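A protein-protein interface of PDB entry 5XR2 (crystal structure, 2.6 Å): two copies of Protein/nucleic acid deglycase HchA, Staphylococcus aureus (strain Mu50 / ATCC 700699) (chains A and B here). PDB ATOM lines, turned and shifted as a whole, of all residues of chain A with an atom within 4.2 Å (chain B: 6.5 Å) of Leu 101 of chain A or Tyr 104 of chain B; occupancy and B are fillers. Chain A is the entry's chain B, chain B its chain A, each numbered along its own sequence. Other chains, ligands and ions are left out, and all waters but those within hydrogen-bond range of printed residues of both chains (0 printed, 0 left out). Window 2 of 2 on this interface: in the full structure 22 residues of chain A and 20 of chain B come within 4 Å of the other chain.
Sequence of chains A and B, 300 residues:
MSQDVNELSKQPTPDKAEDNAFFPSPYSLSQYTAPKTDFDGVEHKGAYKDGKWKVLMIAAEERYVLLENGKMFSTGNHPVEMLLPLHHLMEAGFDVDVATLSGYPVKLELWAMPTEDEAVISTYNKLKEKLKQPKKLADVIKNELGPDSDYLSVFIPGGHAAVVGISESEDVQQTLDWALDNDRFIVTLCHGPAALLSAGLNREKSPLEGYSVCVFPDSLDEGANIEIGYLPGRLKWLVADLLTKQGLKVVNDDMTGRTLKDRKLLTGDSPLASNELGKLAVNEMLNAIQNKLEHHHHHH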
ATOM      1  N   GLU A  61       6.406   3.774  31.071  1.00  0.00           N
ATOM      2  CA  GLU A  61       7.377   2.919  30.348  1.00  0.00           C
ATOM      3  C   GLU A  61       8.660   3.633  29.831  1.00  0.00           C
ATOM      4  O   GLU A  61       9.583   2.945  29.358  1.00  0.00           O
ATOM      5  CB  GLU A  61       6.686   2.179  29.190  1.00  0.00           C
ATOM      6  CG  GLU A  61       6.443   3.014  27.927  1.00  0.00           C
ATOM      7  CD  GLU A  61       5.570   2.323  26.889  1.00  0.00           C
ATOM      8  OE1 GLU A  61       5.256   2.985  25.891  1.00  0.00           O
ATOM      9  OE2 GLU A  61       5.216   1.124  27.035  1.00  0.00           O
ATOM     10  N   GLU A  62       8.710   4.967  29.926  1.00  0.00           N
ATOM     11  CA  GLU A  62       9.875   5.777  29.560  1.00  0.00           C
ATOM     12  C   GLU A  62      10.484   6.443  30.789  1.00  0.00           C
ATOM     13  O   GLU A  62       9.873   7.277  31.396  1.00  0.00           O
ATOM     14  CB  GLU A  62       9.486   6.894  28.547  1.00  0.00           C
ATOM     15  CG  GLU A  62      10.650   7.787  28.061  1.00  0.00           C
ATOM     16  CD  GLU A  62      11.880   6.963  27.701  1.00  0.00           C
ATOM     17  OE1 GLU A  62      12.905   7.044  28.419  1.00  0.00           O
ATOM     18  OE2 GLU A  62      11.810   6.153  26.756  1.00  0.00           O
ATOM     19  N   THR A 100       1.217  -0.844  30.000  1.00  0.00           N
ATOM     20  CA  THR A 100       1.913   0.310  29.500  1.00  0.00           C
ATOM     21  C   THR A 100       1.420   0.626  28.103  1.00  0.00           C
ATOM     22  O   THR A 100       0.703  -0.145  27.498  1.00  0.00           O
ATOM     23  CB  THR A 100       3.437   0.084  29.513  1.00  0.00           C
ATOM     24  OG1 THR A 100       3.805  -1.047  28.689  1.00  0.00           O
ATOM     25  CG2 THR A 100       3.944  -0.118  30.954  1.00  0.00           C
ATOM     26  N   LEU A 101       1.806   1.776  27.576  1.00  0.00           N
ATOM     27  CA  LEU A 101       1.315   2.179  26.271  1.00  0.00           C
ATOM     28  C   LEU A 101       1.797   1.298  25.158  1.00  0.00           C
ATOM     29  O   LEU A 101       1.172   1.308  24.112  1.00  0.00           O
ATOM     30  CB  LEU A 101       1.746   3.594  25.936  1.00  0.00           C
ATOM     31  CG  LEU A 101       1.181   4.691  26.809  1.00  0.00           C
ATOM     32  CD1 LEU A 101       1.715   6.005  26.275  1.00  0.00           C
ATOM     33  CD2 LEU A 101      -0.346   4.645  26.830  1.00  0.00           C
ATOM     34  N   SER A 102       2.930   0.597  25.355  1.00  0.00           N
ATOM     35  CA  SER A 102       3.524  -0.265  24.328  1.00  0.00           C
ATOM     36  C   SER A 102       3.771  -1.708  24.771  1.00  0.00           C
ATOM     37  O   SER A 102       4.164  -2.505  23.946  1.00  0.00           O
ATOM     38  CB  SER A 102       4.854   0.321  23.849  1.00  0.00           C
ATOM     39  OG  SER A 102       4.782   1.730  23.601  1.00  0.00           O
ATOM     40  N   GLY A 103       3.525  -2.069  26.027  1.00  0.00           N
ATOM     41  CA  GLY A 103       3.943  -3.376  26.530  1.00  0.00           C
ATOM     42  C   GLY A 103       5.395  -3.417  26.970  1.00  0.00           C
ATOM     43  O   GLY A 103       5.919  -4.471  27.242  1.00  0.00           O
ATOM     44  N   LEU A 137      -1.721  -1.570  26.524  1.00  0.00           N
ATOM     45  CA  LEU A 137      -2.962  -0.854  26.773  1.00  0.00           C
ATOM     46  C   LEU A 137      -3.977  -0.901  25.635  1.00  0.00           C
ATOM     47  O   LEU A 137      -5.175  -0.861  25.896  1.00  0.00           O
ATOM     48  CB  LEU A 137      -2.687   0.621  27.134  1.00  0.00           C
ATOM     49  CG  LEU A 137      -3.911   1.436  27.612  1.00  0.00           C
ATOM     50  CD1 LEU A 137      -4.553   0.747  28.804  1.00  0.00           C
ATOM     51  CD2 LEU A 137      -3.608   2.878  27.950  1.00  0.00           C
ATOM     52  N   GLY A 165       4.477  10.663  27.262  1.00  0.00           N
ATOM     53  CA  GLY A 165       3.642   9.661  26.544  1.00  0.00           C
ATOM     54  C   GLY A 165       2.204   9.456  27.043  1.00  0.00           C
ATOM     55  O   GLY A 165       1.265   9.516  26.267  1.00  0.00           O
ATOM     56  N   ILE A 166       2.047   9.174  28.337  1.00  0.00           N
ATOM     57  CA  ILE A 166       0.746   9.095  29.033  1.00  0.00           C
ATOM     58  C   ILE A 166      -0.069  10.407  29.024  1.00  0.00           C
ATOM     59  O   ILE A 166      -1.291  10.361  29.155  1.00  0.00           O
ATOM     60  CB  ILE A 166       0.994   8.568  30.474  1.00  0.00           C
ATOM     61  CG1 ILE A 166       1.283   7.067  30.412  1.00  0.00           C
ATOM     62  CG2 ILE A 166      -0.148   8.828  31.445  1.00  0.00           C
ATOM     63  CD1 ILE A 166       1.905   6.511  31.684  1.00  0.00           C
ATOM     64  N   SER A 169      -1.845  10.582  24.842  1.00  0.00           N
ATOM     65  CA  SER A 169      -2.144   9.280  24.303  1.00  0.00           C
ATOM     66  C   SER A 169      -3.641   9.137  24.044  1.00  0.00           C
ATOM     67  O   SER A 169      -4.460   9.351  24.945  1.00  0.00           O
ATOM     68  CB  SER A 169      -1.699   8.221  25.308  1.00  0.00           C
ATOM     69  OG  SER A 169      -2.359   6.996  25.060  1.00  0.00           O
ATOM     70  N   VAL A 172      -4.856   6.232  26.259  1.00  0.00           N
ATOM     71  CA  VAL A 172      -5.233   6.692  27.624  1.00  0.00           C
ATOM     72  C   VAL A 172      -6.593   7.420  27.566  1.00  0.00           C
ATOM     73  O   VAL A 172      -7.485   7.109  28.343  1.00  0.00           O
ATOM     74  CB  VAL A 172      -4.140   7.560  28.312  1.00  0.00           C
ATOM     75  CG1 VAL A 172      -4.673   8.212  29.574  1.00  0.00           C
ATOM     76  CG2 VAL A 172      -2.946   6.709  28.664  1.00  0.00           C
ATOM     77  N   ALA B  60      15.395   1.990  18.164  1.00  0.00           N
ATOM     78  CA  ALA B  60      14.863   1.342  19.335  1.00  0.00           C
ATOM     79  C   ALA B  60      14.685   2.374  20.451  1.00  0.00           C
ATOM     80  O   ALA B  60      15.461   3.334  20.564  1.00  0.00           O
ATOM     81  CB  ALA B  60      15.792   0.214  19.744  1.00  0.00           C
ATOM     82  N   GLU B  61      13.610   2.225  21.218  1.00  0.00           N
ATOM     83  CA  GLU B  61      13.292   3.165  22.308  1.00  0.00           C
ATOM     84  C   GLU B  61      13.207   2.460  23.667  1.00  0.00           C
ATOM     85  O   GLU B  61      13.072   3.120  24.691  1.00  0.00           O
ATOM     86  CB  GLU B  61      11.999   3.971  22.001  1.00  0.00           C
ATOM     87  CG  GLU B  61      10.729   3.132  22.102  1.00  0.00           C
ATOM     88  CD  GLU B  61       9.425   3.808  21.669  1.00  0.00           C
ATOM     89  OE1 GLU B  61       9.363   5.059  21.486  1.00  0.00           O
ATOM     90  OE2 GLU B  61       8.431   3.034  21.544  1.00  0.00           O
ATOM     91  N   GLU B  62      13.321   1.142  23.686  1.00  0.00           N
ATOM     92  CA  GLU B  62      13.452   0.390  24.926  1.00  0.00           C
ATOM     93  C   GLU B  62      14.882  -0.119  25.034  1.00  0.00           C
ATOM     94  O   GLU B  62      15.389  -0.675  24.111  1.00  0.00           O
ATOM     95  CB  GLU B  62      12.480  -0.766  24.924  1.00  0.00           C
ATOM     96  CG  GLU B  62      12.538  -1.662  26.154  1.00  0.00           C
ATOM     97  CD  GLU B  62      12.336  -0.887  27.430  1.00  0.00           C
ATOM     98  OE1 GLU B  62      13.149  -1.074  28.376  1.00  0.00           O
ATOM     99  OE2 GLU B  62      11.392  -0.075  27.446  1.00  0.00           O
ATOM    100  N   ALA B  99      12.737   8.040  13.678  1.00  0.00           N
ATOM    101  CA  ALA B  99      11.471   7.711  14.300  1.00  0.00           C
ATOM    102  C   ALA B  99      11.611   6.541  15.280  1.00  0.00           C
ATOM    103  O   ALA B  99      12.488   5.690  15.153  1.00  0.00           O
ATOM    104  CB  ALA B  99      10.437   7.391  13.243  1.00  0.00           C
ATOM    105  N   THR B 100      10.748   6.556  16.287  1.00  0.00           N
ATOM    106  CA  THR B 100      10.565   5.461  17.192  1.00  0.00           C
ATOM    107  C   THR B 100       9.070   5.194  17.244  1.00  0.00           C
ATOM    108  O   THR B 100       8.264   5.909  16.610  1.00  0.00           O
ATOM    109  CB  THR B 100      11.151   5.769  18.580  1.00  0.00           C
ATOM    110  OG1 THR B 100      10.604   6.969  19.126  1.00  0.00           O
ATOM    111  CG2 THR B 100      12.621   5.954  18.492  1.00  0.00           C
ATOM    112  N   LEU B 101       8.690   4.146  17.962  1.00  0.00           N
ATOM    113  CA  LEU B 101       7.301   3.737  17.966  1.00  0.00           C
ATOM    114  C   LEU B 101       6.411   4.648  18.788  1.00  0.00           C
ATOM    115  O   LEU B 101       5.208   4.664  18.566  1.00  0.00           O
ATOM    116  CB  LEU B 101       7.154   2.295  18.440  1.00  0.00           C
ATOM    117  CG  LEU B 101       7.822   1.250  17.598  1.00  0.00           C
ATOM    118  CD1 LEU B 101       7.315  -0.114  17.985  1.00  0.00           C
ATOM    119  CD2 LEU B 101       7.525   1.511  16.136  1.00  0.00           C
ATOM    120  N   SER B 102       6.965   5.390  19.731  1.00  0.00           N
ATOM    121  CA  SER B 102       6.150   6.297  20.525  1.00  0.00           C
ATOM    122  C   SER B 102       6.689   7.700  20.515  1.00  0.00           C
ATOM    123  O   SER B 102       6.106   8.556  21.118  1.00  0.00           O
ATOM    124  CB  SER B 102       6.096   5.806  21.953  1.00  0.00           C
ATOM    125  OG  SER B 102       5.965   4.398  22.004  1.00  0.00           O
ATOM    126  N   GLY B 103       7.778   7.960  19.812  1.00  0.00           N
ATOM    127  CA  GLY B 103       8.430   9.234  19.921  1.00  0.00           C
ATOM    128  C   GLY B 103       9.209   9.412  21.206  1.00  0.00           C
ATOM    129  O   GLY B 103       9.616  10.522  21.502  1.00  0.00           O
ATOM    130  N   TYR B 104       9.485   8.330  21.937  1.00  0.00           N
ATOM    131  CA  TYR B 104      10.392   8.415  23.085  1.00  0.00           C
ATOM    132  C   TYR B 104      11.832   8.561  22.556  1.00  0.00           C
ATOM    133  O   TYR B 104      12.083   8.249  21.381  1.00  0.00           O
ATOM    134  CB  TYR B 104      10.339   7.167  23.969  1.00  0.00           C
ATOM    135  CG  TYR B 104       9.006   6.772  24.563  1.00  0.00           C
ATOM    136  CD1 TYR B 104       8.053   7.715  24.950  1.00  0.00           C
ATOM    137  CD2 TYR B 104       8.706   5.437  24.759  1.00  0.00           C
ATOM    138  CE1 TYR B 104       6.835   7.326  25.500  1.00  0.00           C
ATOM    139  CE2 TYR B 104       7.487   5.039  25.295  1.00  0.00           C
ATOM    140  CZ  TYR B 104       6.560   5.989  25.671  1.00  0.00           C
ATOM    141  OH  TYR B 104       5.372   5.596  26.203  1.00  0.00           O
ATOM    142  N   PRO B 105      12.781   8.998  23.427  1.00  0.00           N
ATOM    143  CA  PRO B 105      14.190   9.080  23.027  1.00  0.00           C
ATOM    144  C   PRO B 105      14.803   7.733  22.639  1.00  0.00           C
ATOM    145  O   PRO B 105      14.407   6.702  23.159  1.00  0.00           O
ATOM    146  CB  PRO B 105      14.888   9.619  24.288  1.00  0.00           C
ATOM    147  CG  PRO B 105      13.792  10.238  25.094  1.00  0.00           C
ATOM    148  CD  PRO B 105      12.631   9.337  24.857  1.00  0.00           C
ATOM    149  N   VAL B 106      15.775   7.785  21.735  1.00  0.00           N
ATOM    150  CA  VAL B 106      16.474   6.631  21.239  1.00  0.00           C
ATOM    151  C   VAL B 106      17.418   6.112  22.310  1.00  0.00           C
ATOM    152  O   VAL B 106      18.144   6.875  22.909  1.00  0.00           O
ATOM    153  CB  VAL B 106      17.255   6.984  19.982  1.00  0.00           C
ATOM    154  CG1 VAL B 106      18.196   5.854  19.580  1.00  0.00           C
ATOM    155  CG2 VAL B 106      16.267   7.309  18.854  1.00  0.00           C
ATOM    156  N   LYS B 107      17.377   4.801  22.547  1.00  0.00           N
ATOM    157  CA  LYS B 107      18.231   4.140  23.505  1.00  0.00           C
ATOM    158  C   LYS B 107      19.426   3.536  22.766  1.00  0.00           C
ATOM    159  O   LYS B 107      19.254   2.634  21.972  1.00  0.00           O
ATOM    160  CB  LYS B 107      17.440   3.069  24.234  1.00  0.00           C
ATOM    161  CG  LYS B 107      16.166   3.589  24.879  1.00  0.00           C
ATOM    162  CD  LYS B 107      16.433   4.653  25.924  1.00  0.00           C
ATOM    163  CE  LYS B 107      15.146   5.152  26.552  1.00  0.00           C
ATOM    164  NZ  LYS B 107      14.170   5.708  25.579  1.00  0.00           N
ATOM    165  N   LEU B 131      17.777  12.234  17.823  1.00  0.00           N
ATOM    166  CA  LEU B 131      17.787  11.042  18.640  1.00  0.00           C
ATOM    167  C   LEU B 131      17.036  11.258  19.963  1.00  0.00           C
ATOM    168  O   LEU B 131      16.378  10.331  20.464  1.00  0.00           O
ATOM    169  CB  LEU B 131      19.227  10.585  18.933  1.00  0.00           C
ATOM    170  CG  LEU B 131      20.076  10.187  17.716  1.00  0.00           C
ATOM    171  CD1 LEU B 131      21.534  10.028  18.120  1.00  0.00           C
ATOM    172  CD2 LEU B 131      19.591   8.933  17.016  1.00  0.00           C
ATOM    173  N   LYS B 132      17.141  12.461  20.528  1.00  0.00           N
ATOM    174  CA  LYS B 132      16.469  12.790  21.810  1.00  0.00           C
ATOM    175  C   LYS B 132      14.969  13.160  21.650  1.00  0.00           C
ATOM    176  O   LYS B 132      14.194  12.990  22.600  1.00  0.00           O
ATOM    177  CB  LYS B 132      17.224  13.903  22.569  1.00  0.00           C
ATOM    178  CG  LYS B 132      18.701  13.598  22.775  1.00  0.00           C
ATOM    179  CD  LYS B 132      19.219  13.957  24.158  1.00  0.00           C
ATOM    180  CE  LYS B 132      20.469  13.139  24.434  1.00  0.00           C
ATOM    181  NZ  LYS B 132      20.955  13.435  25.787  1.00  0.00           N
ATOM    182  N   GLN B 133      14.584  13.654  20.461  1.00  0.00           N
ATOM    183  CA  GLN B 133      13.189  13.960  20.147  1.00  0.00           C
ATOM    184  C   GLN B 133      12.815  13.449  18.765  1.00  0.00           C
ATOM    185  O   GLN B 133      12.689  14.212  17.813  1.00  0.00           O
ATOM    186  CB  GLN B 133      12.945  15.454  20.213  1.00  0.00           C
ATOM    187  CG  GLN B 133      12.626  16.018  21.571  1.00  0.00           C
ATOM    188  CD  GLN B 133      12.441  17.524  21.458  1.00  0.00           C
ATOM    189  OE1 GLN B 133      11.335  18.038  21.559  1.00  0.00           O
ATOM    190  NE2 GLN B 133      13.537  18.231  21.183  1.00  0.00           N
ATOM    191  N   PRO B 134      12.630  12.138  18.644  1.00  0.00           N
ATOM    192  CA  PRO B 134      12.358  11.600  17.321  1.00  0.00           C
ATOM    193  C   PRO B 134      10.940  11.879  16.878  1.00  0.00           C
ATOM    194  O   PRO B 134      10.107  12.220  17.708  1.00  0.00           O
ATOM    195  CB  PRO B 134      12.547  10.080  17.523  1.00  0.00           C
ATOM    196  CG  PRO B 134      13.274   9.942  18.812  1.00  0.00           C
ATOM    197  CD  PRO B 134      12.753  11.061  19.639  1.00  0.00           C
ATOM    198  N   LYS B 135      10.661  11.693  15.593  1.00  0.00           N
ATOM    199  CA  LYS B 135       9.282  11.690  15.136  1.00  0.00           C
ATOM    200  C   LYS B 135       8.605  10.433  15.666  1.00  0.00           C
ATOM    201  O   LYS B 135       9.280   9.541  16.163  1.00  0.00           O
ATOM    202  CB  LYS B 135       9.207  11.702  13.619  1.00  0.00           C
ATOM    203  CG  LYS B 135       9.845  12.893  12.917  1.00  0.00           C
ATOM    204  CD  LYS B 135       9.704  12.676  11.415  1.00  0.00           C
ATOM    205  CE  LYS B 135      10.585  13.590  10.595  1.00  0.00           C
ATOM    206  NZ  LYS B 135       9.846  14.788  10.141  1.00  0.00           N
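O of Glu 61 of chain B touches OE2 of Glu 62 of chain A, 3.9 Å away. CB of Tyr 104 of chain B touches OE2 of Glu 62 of chain A, 3.3 Å away. Glu 62 of chain A touches Pro 105 of chain B (CD to CD, 3.8 Å). Leu 101 of chain A touches Tyr 104 of chain B (CD1 to OH, 3.7 Å).
The backbone carbonyl oxygen (O) of Ala 60 of chain B sits at hydrogen-bond distance from the backbone NH (N) of Lys 107 of chain B (3.1 Å). OG1 of Thr 100 of chain B is in hydrogen-bond range of OE1 of Glu 61 of chain B, at 3.3 Å. N of Tyr 104 of chain B is in hydrogen-bond range of OE1 of Glu 61 of chain B (3.3 Å). The side-chain hydroxyl of Thr 100 of chain B sits at hydrogen-bond distance from the backbone carbonyl oxygen of Tyr 104 of chain B (3.0 Å). The side-chain amino group (NZ) of Lys 107 of chain B sits at hydrogen-bond distance from the backbone carbonyl oxygen (O) of Pro 105 of chain B. OE1 of Glu 61 of chain A is in hydrogen-bond range of OG of Ser 102 of chain A, at 2.7 Å.
Leu 101 of chain A touches just one residue of chain B: Tyr 104. Of the printed residues of chain B, Glu 62 of chain A touches Glu 61 (3.9 Å), Tyr 104 (3.3 Å), Pro 105 (3.8 Å) and Lys 107 (2.7 Å). Of the printed residues of chain A, Ser 102 of chain B touches Ser 102. Printed residues of chain B within 4 Å of Glu 61 of chain A: Tyr 104. The nearest residue of chain A that does not touch Tyr 104 of chain B is Gly 165 of chain A (4.1 Å).
Of the 11 printed residues of chain A, 4 touch a printed residue of chain B. Along chain B the printed residues that touch a printed residue of chain A span positions 61 to 107. Among the printed residues, Asp or Glu carboxylates within 4 Å of a Lys or Arg side-chain nitrogen of the other chain: Glu 62 of chain A with Lys 107 of chain B.
Glu 62 of chain A touches Glu 61 of chain B, but with the chains exchanged Glu 61 of chain A does not touch Glu 62 of chain B (4.01 Å). Ser 102 of chain A touches its own counterpart, Ser 102 of chain B. Positions printed for both chains: 61, 62, 100, 101, 102 and 103.
OG of Ser 102 of chain B sits at hydrogen-bond distance from OG of Ser 102 of chain A (3.3 Å). The side-chain hydroxyl of Tyr 104 of chain B lies within hydrogen-bond range of the side-chain carboxylate of Glu 61 of chain A (2.6 Å). OE2 of Glu 62 of chain A is in salt-bridge range of NZ of Lys 107 of chain B (2.7 Å).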
